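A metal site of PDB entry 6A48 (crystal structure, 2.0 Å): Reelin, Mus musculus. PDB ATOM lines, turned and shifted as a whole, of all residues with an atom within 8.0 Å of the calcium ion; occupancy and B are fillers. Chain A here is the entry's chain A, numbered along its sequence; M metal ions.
The backbone carbonyl oxygen (O) of Glu 600 sits at hydrogen-bond distance from the side-chain amide nitrogen (NE2) of Gln 650 (2.7 Å). N of Asp 659 lies within hydrogen-bond range of O of Arg 593, at 3.3 Å. The side-chain carboxylate (OE2) of Glu 600 lies close to the backbone NH (N) of Gln 597. O of Asp 659 is in hydrogen-bond range of NE2 of Gln 650 (3.1 Å).
Of the 17 residues printed, 4 come within 4 Å of the calcium ion. The nearest printed residue that does not touch the calcium ion is Gln 597 (4.3 Å).
The calcium ion is bound by OD2 of Asp 596 (2.4 Å), OE1 of Glu 600 (2.4 Å), OG of Ser 654 (2.4 Å), OE2 of Glu 600 (2.6 Å), OD1 of Asp 659 (2.8 Å) and OD2 of Asp 659 (2.8 Å).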
ATOM      1  N   ARG A 593      -5.756 -15.228 -27.360  1.00  0.00           N
ATOM      2  CA  ARG A 593      -6.146 -16.610 -27.100  1.00  0.00           C
ATOM      3  C   ARG A 593      -7.184 -16.662 -25.988  1.00  0.00           C
ATOM      4  O   ARG A 593      -7.050 -16.010 -24.952  1.00  0.00           O
ATOM      5  CB  ARG A 593      -4.917 -17.449 -26.757  1.00  0.00           C
ATOM      6  CG  ARG A 593      -4.143 -17.857 -28.016  1.00  0.00           C
ATOM      7  CD  ARG A 593      -2.803 -18.507 -27.707  1.00  0.00           C
ATOM      8  NE  ARG A 593      -1.794 -17.527 -27.315  1.00  0.00           N
ATOM      9  CZ  ARG A 593      -1.401 -17.331 -26.056  1.00  0.00           C
ATOM     10  NH1 ARG A 593      -1.925 -18.067 -25.081  1.00  0.00           N
ATOM     11  NH2 ARG A 593      -0.471 -16.420 -25.789  1.00  0.00           N
ATOM     12  N   ALA A 594      -8.230 -17.461 -26.216  1.00  0.00           N
ATOM     13  CA  ALA A 594      -9.439 -17.388 -25.420  1.00  0.00           C
ATOM     14  C   ALA A 594      -9.212 -17.849 -23.983  1.00  0.00           C
ATOM     15  O   ALA A 594      -8.318 -18.668 -23.710  1.00  0.00           O
ATOM     16  CB  ALA A 594     -10.528 -18.246 -26.054  1.00  0.00           C
ATOM     17  N   PRO A 595      -9.984 -17.331 -23.039  1.00  0.00           N
ATOM     18  CA  PRO A 595      -9.999 -17.906 -21.683  1.00  0.00           C
ATOM     19  C   PRO A 595     -10.374 -19.377 -21.736  1.00  0.00           C
ATOM     20  O   PRO A 595     -11.376 -19.761 -22.349  1.00  0.00           O
ATOM     21  CB  PRO A 595     -11.060 -17.060 -20.961  1.00  0.00           C
ATOM     22  CG  PRO A 595     -11.132 -15.784 -21.726  1.00  0.00           C
ATOM     23  CD  PRO A 595     -10.862 -16.151 -23.148  1.00  0.00           C
ATOM     24  N   ASP A 596      -9.563 -20.200 -21.064  1.00  0.00           N
ATOM     25  CA  ASP A 596      -9.729 -21.647 -21.130  1.00  0.00           C
ATOM     26  C   ASP A 596     -10.309 -22.263 -19.870  1.00  0.00           C
ATOM     27  O   ASP A 596     -10.664 -23.439 -19.892  1.00  0.00           O
ATOM     28  CB  ASP A 596      -8.381 -22.317 -21.448  1.00  0.00           C
ATOM     29  CG  ASP A 596      -7.252 -21.826 -20.570  1.00  0.00           C
ATOM     30  OD1 ASP A 596      -6.097 -21.789 -21.044  1.00  0.00           O
ATOM     31  OD2 ASP A 596      -7.509 -21.471 -19.401  1.00  0.00           O
ATOM     32  N   GLN A 597     -10.428 -21.507 -18.776  1.00  0.00           N
ATOM     33  CA  GLN A 597     -10.907 -22.113 -17.543  1.00  0.00           C
ATOM     34  C   GLN A 597     -12.168 -21.432 -17.043  1.00  0.00           C
ATOM     35  O   GLN A 597     -12.370 -20.234 -17.268  1.00  0.00           O
ATOM     36  CB  GLN A 597      -9.826 -22.070 -16.455  1.00  0.00           C
ATOM     37  CG  GLN A 597      -8.739 -23.100 -16.646  1.00  0.00           C
ATOM     38  CD  GLN A 597      -9.297 -24.500 -16.863  1.00  0.00           C
ATOM     39  OE1 GLN A 597      -9.071 -25.107 -17.908  1.00  0.00           O
ATOM     40  NE2 GLN A 597     -10.035 -24.995 -15.880  1.00  0.00           N
ATOM     41  N   PRO A 598     -13.060 -22.180 -16.381  1.00  0.00           N
ATOM     42  CA  PRO A 598     -14.220 -21.568 -15.731  1.00  0.00           C
ATOM     43  C   PRO A 598     -13.821 -20.387 -14.852  1.00  0.00           C
ATOM     44  O   PRO A 598     -12.723 -20.351 -14.295  1.00  0.00           O
ATOM     45  CB  PRO A 598     -14.804 -22.713 -14.896  1.00  0.00           C
ATOM     46  CG  PRO A 598     -14.236 -23.982 -15.477  1.00  0.00           C
ATOM     47  CD  PRO A 598     -13.178 -23.645 -16.486  1.00  0.00           C
ATOM     48  N   GLU A 600     -12.998 -17.511 -15.761  1.00  0.00           N
ATOM     49  CA  GLU A 600     -12.154 -16.560 -16.471  1.00  0.00           C
ATOM     50  C   GLU A 600     -12.952 -15.707 -17.448  1.00  0.00           C
ATOM     51  O   GLU A 600     -12.361 -15.039 -18.302  1.00  0.00           O
ATOM     52  CB  GLU A 600     -11.034 -17.291 -17.210  1.00  0.00           C
ATOM     53  CG  GLU A 600     -10.123 -18.095 -16.282  1.00  0.00           C
ATOM     54  CD  GLU A 600      -8.891 -18.646 -16.985  1.00  0.00           C
ATOM     55  OE1 GLU A 600      -7.791 -18.498 -16.431  1.00  0.00           O
ATOM     56  OE2 GLU A 600      -9.046 -19.218 -18.081  1.00  0.00           O
ATOM     57  N   TYR A 622     -16.813 -17.742 -20.205  1.00  0.00           N
ATOM     58  CA  TYR A 622     -15.562 -17.893 -20.942  1.00  0.00           C
ATOM     59  C   TYR A 622     -15.757 -18.791 -22.170  1.00  0.00           C
ATOM     60  O   TYR A 622     -14.779 -19.116 -22.855  1.00  0.00           O
ATOM     61  CB  TYR A 622     -14.480 -18.455 -20.019  1.00  0.00           C
ATOM     62  CG  TYR A 622     -14.599 -19.958 -19.771  1.00  0.00           C
ATOM     63  CD1 TYR A 622     -15.574 -20.472 -18.928  1.00  0.00           C
ATOM     64  CD2 TYR A 622     -13.732 -20.845 -20.394  1.00  0.00           C
ATOM     65  CE1 TYR A 622     -15.689 -21.841 -18.709  1.00  0.00           C
ATOM     66  CE2 TYR A 622     -13.830 -22.204 -20.174  1.00  0.00           C
ATOM     67  CZ  TYR A 622     -14.808 -22.691 -19.344  1.00  0.00           C
ATOM     68  OH  TYR A 622     -14.903 -24.053 -19.146  1.00  0.00           O
ATOM     69  N   GLN A 650     -12.455  -8.876 -15.505  1.00  0.00           N
ATOM     70  CA  GLN A 650     -12.115 -10.290 -15.565  1.00  0.00           C
ATOM     71  C   GLN A 650     -11.399 -10.637 -14.265  1.00  0.00           C
ATOM     72  O   GLN A 650     -10.202 -10.351 -14.119  1.00  0.00           O
ATOM     73  CB  GLN A 650     -11.216 -10.601 -16.768  1.00  0.00           C
ATOM     74  CG  GLN A 650     -10.848 -12.076 -16.887  1.00  0.00           C
ATOM     75  CD  GLN A 650      -9.949 -12.368 -18.074  1.00  0.00           C
ATOM     76  OE1 GLN A 650      -9.046 -11.599 -18.390  1.00  0.00           O
ATOM     77  NE2 GLN A 650     -10.187 -13.492 -18.735  1.00  0.00           N
ATOM     78  N   TYR A 652     -10.456 -13.532 -12.849  1.00  0.00           N
ATOM     79  CA  TYR A 652      -9.494 -14.622 -12.900  1.00  0.00           C
ATOM     80  C   TYR A 652      -8.920 -14.758 -14.300  1.00  0.00           C
ATOM     81  O   TYR A 652      -9.676 -14.791 -15.279  1.00  0.00           O
ATOM     82  CB  TYR A 652     -10.127 -15.949 -12.481  1.00  0.00           C
ATOM     83  CG  TYR A 652     -10.771 -15.946 -11.109  1.00  0.00           C
ATOM     84  CD1 TYR A 652     -10.027 -15.679  -9.966  1.00  0.00           C
ATOM     85  CD2 TYR A 652     -12.125 -16.239 -10.954  1.00  0.00           C
ATOM     86  CE1 TYR A 652     -10.611 -15.686  -8.716  1.00  0.00           C
ATOM     87  CE2 TYR A 652     -12.722 -16.240  -9.712  1.00  0.00           C
ATOM     88  CZ  TYR A 652     -11.958 -15.966  -8.589  1.00  0.00           C
ATOM     89  OH  TYR A 652     -12.551 -15.975  -7.349  1.00  0.00           O
ATOM     90  N   HIS A 653      -7.594 -14.853 -14.397  1.00  0.00           N
ATOM     91  CA  HIS A 653      -6.926 -15.143 -15.657  1.00  0.00           C
ATOM     92  C   HIS A 653      -5.514 -15.619 -15.372  1.00  0.00           C
ATOM     93  O   HIS A 653      -4.979 -15.407 -14.277  1.00  0.00           O
ATOM     94  CB  HIS A 653      -6.909 -13.919 -16.589  1.00  0.00           C
ATOM     95  CG  HIS A 653      -6.273 -12.710 -15.992  1.00  0.00           C
ATOM     96  ND1 HIS A 653      -4.916 -12.499 -15.993  1.00  0.00           N
ATOM     97  CD2 HIS A 653      -6.821 -11.636 -15.370  1.00  0.00           C
ATOM     98  CE1 HIS A 653      -4.640 -11.353 -15.403  1.00  0.00           C
ATOM     99  NE2 HIS A 653      -5.778 -10.804 -15.019  1.00  0.00           N
ATOM    100  N   SER A 654      -4.908 -16.262 -16.366  1.00  0.00           N
ATOM    101  CA  SER A 654      -3.587 -16.862 -16.219  1.00  0.00           C
ATOM    102  C   SER A 654      -2.448 -15.863 -16.372  1.00  0.00           C
ATOM    103  O   SER A 654      -1.278 -16.277 -16.340  1.00  0.00           O
ATOM    104  CB  SER A 654      -3.425 -18.013 -17.211  1.00  0.00           C
ATOM    105  OG  SER A 654      -4.465 -18.964 -17.054  1.00  0.00           O
ATOM    106  N   SER A 655      -2.759 -14.584 -16.567  1.00  0.00           N
ATOM    107  CA  SER A 655      -1.831 -13.471 -16.331  1.00  0.00           C
ATOM    108  C   SER A 655      -0.526 -13.611 -17.111  1.00  0.00           C
ATOM    109  O   SER A 655       0.570 -13.650 -16.552  1.00  0.00           O
ATOM    110  CB  SER A 655      -1.551 -13.310 -14.833  1.00  0.00           C
ATOM    111  OG  SER A 655      -0.838 -14.436 -14.323  1.00  0.00           O
ATOM    112  N   GLN A 656      -0.653 -13.658 -18.438  1.00  0.00           N
ATOM    113  CA  GLN A 656       0.502 -13.614 -19.324  1.00  0.00           C
ATOM    114  C   GLN A 656       0.135 -12.824 -20.571  1.00  0.00           C
ATOM    115  O   GLN A 656       0.071 -11.592 -20.551  1.00  0.00           O
ATOM    116  CB  GLN A 656       0.973 -15.013 -19.722  1.00  0.00           C
ATOM    117  CG  GLN A 656       1.324 -15.942 -18.571  1.00  0.00           C
ATOM    118  CD  GLN A 656       1.404 -17.408 -18.984  1.00  0.00           C
ATOM    119  OE1 GLN A 656       1.800 -17.728 -20.104  1.00  0.00           O
ATOM    120  NE2 GLN A 656       1.017 -18.305 -18.082  1.00  0.00           N
ATOM    121  N   GLU A 658      -2.545 -14.438 -21.882  1.00  0.00           N
ATOM    122  CA  GLU A 658      -3.509 -15.523 -21.849  1.00  0.00           C
ATOM    123  C   GLU A 658      -4.908 -15.003 -21.502  1.00  0.00           C
ATOM    124  O   GLU A 658      -5.066 -13.954 -20.879  1.00  0.00           O
ATOM    125  CB  GLU A 658      -3.103 -16.584 -20.830  1.00  0.00           C
ATOM    126  CG  GLU A 658      -1.654 -17.001 -20.937  1.00  0.00           C
ATOM    127  CD  GLU A 658      -1.481 -18.514 -20.934  1.00  0.00           C
ATOM    128  OE1 GLU A 658      -1.298 -19.084 -22.028  1.00  0.00           O
ATOM    129  OE2 GLU A 658      -1.541 -19.120 -19.841  1.00  0.00           O
ATOM    130  N   ASP A 659      -5.910 -15.778 -21.915  1.00  0.00           N
ATOM    131  CA  ASP A 659      -7.304 -15.518 -21.583  1.00  0.00           C
ATOM    132  C   ASP A 659      -7.705 -14.103 -22.005  1.00  0.00           C
ATOM    133  O   ASP A 659      -8.425 -13.394 -21.296  1.00  0.00           O
ATOM    134  CB  ASP A 659      -7.560 -15.747 -20.097  1.00  0.00           C
ATOM    135  CG  ASP A 659      -6.940 -17.048 -19.603  1.00  0.00           C
ATOM    136  OD1 ASP A 659      -7.173 -18.105 -20.237  1.00  0.00           O
ATOM    137  OD2 ASP A 659      -6.200 -17.011 -18.590  1.00  0.00           O
ATOM    138  N   VAL A 660      -7.209 -13.691 -23.165  1.00  0.00           N
ATOM    139  CA  VAL A 660      -7.383 -12.317 -23.627  1.00  0.00           C
ATOM    140  C   VAL A 660      -8.838 -12.089 -24.023  1.00  0.00           C
ATOM    141  O   VAL A 660      -9.486 -12.966 -24.617  1.00  0.00           O
ATOM    142  CB  VAL A 660      -6.416 -12.027 -24.786  1.00  0.00           C
ATOM    143  CG1 VAL A 660      -6.565 -10.598 -25.257  1.00  0.00           C
ATOM    144  CG2 VAL A 660      -4.986 -12.313 -24.371  1.00  0.00           C
HETATM  145 CA    CA M   1      -6.541 -19.729 -18.086  1.00  0.00          CA
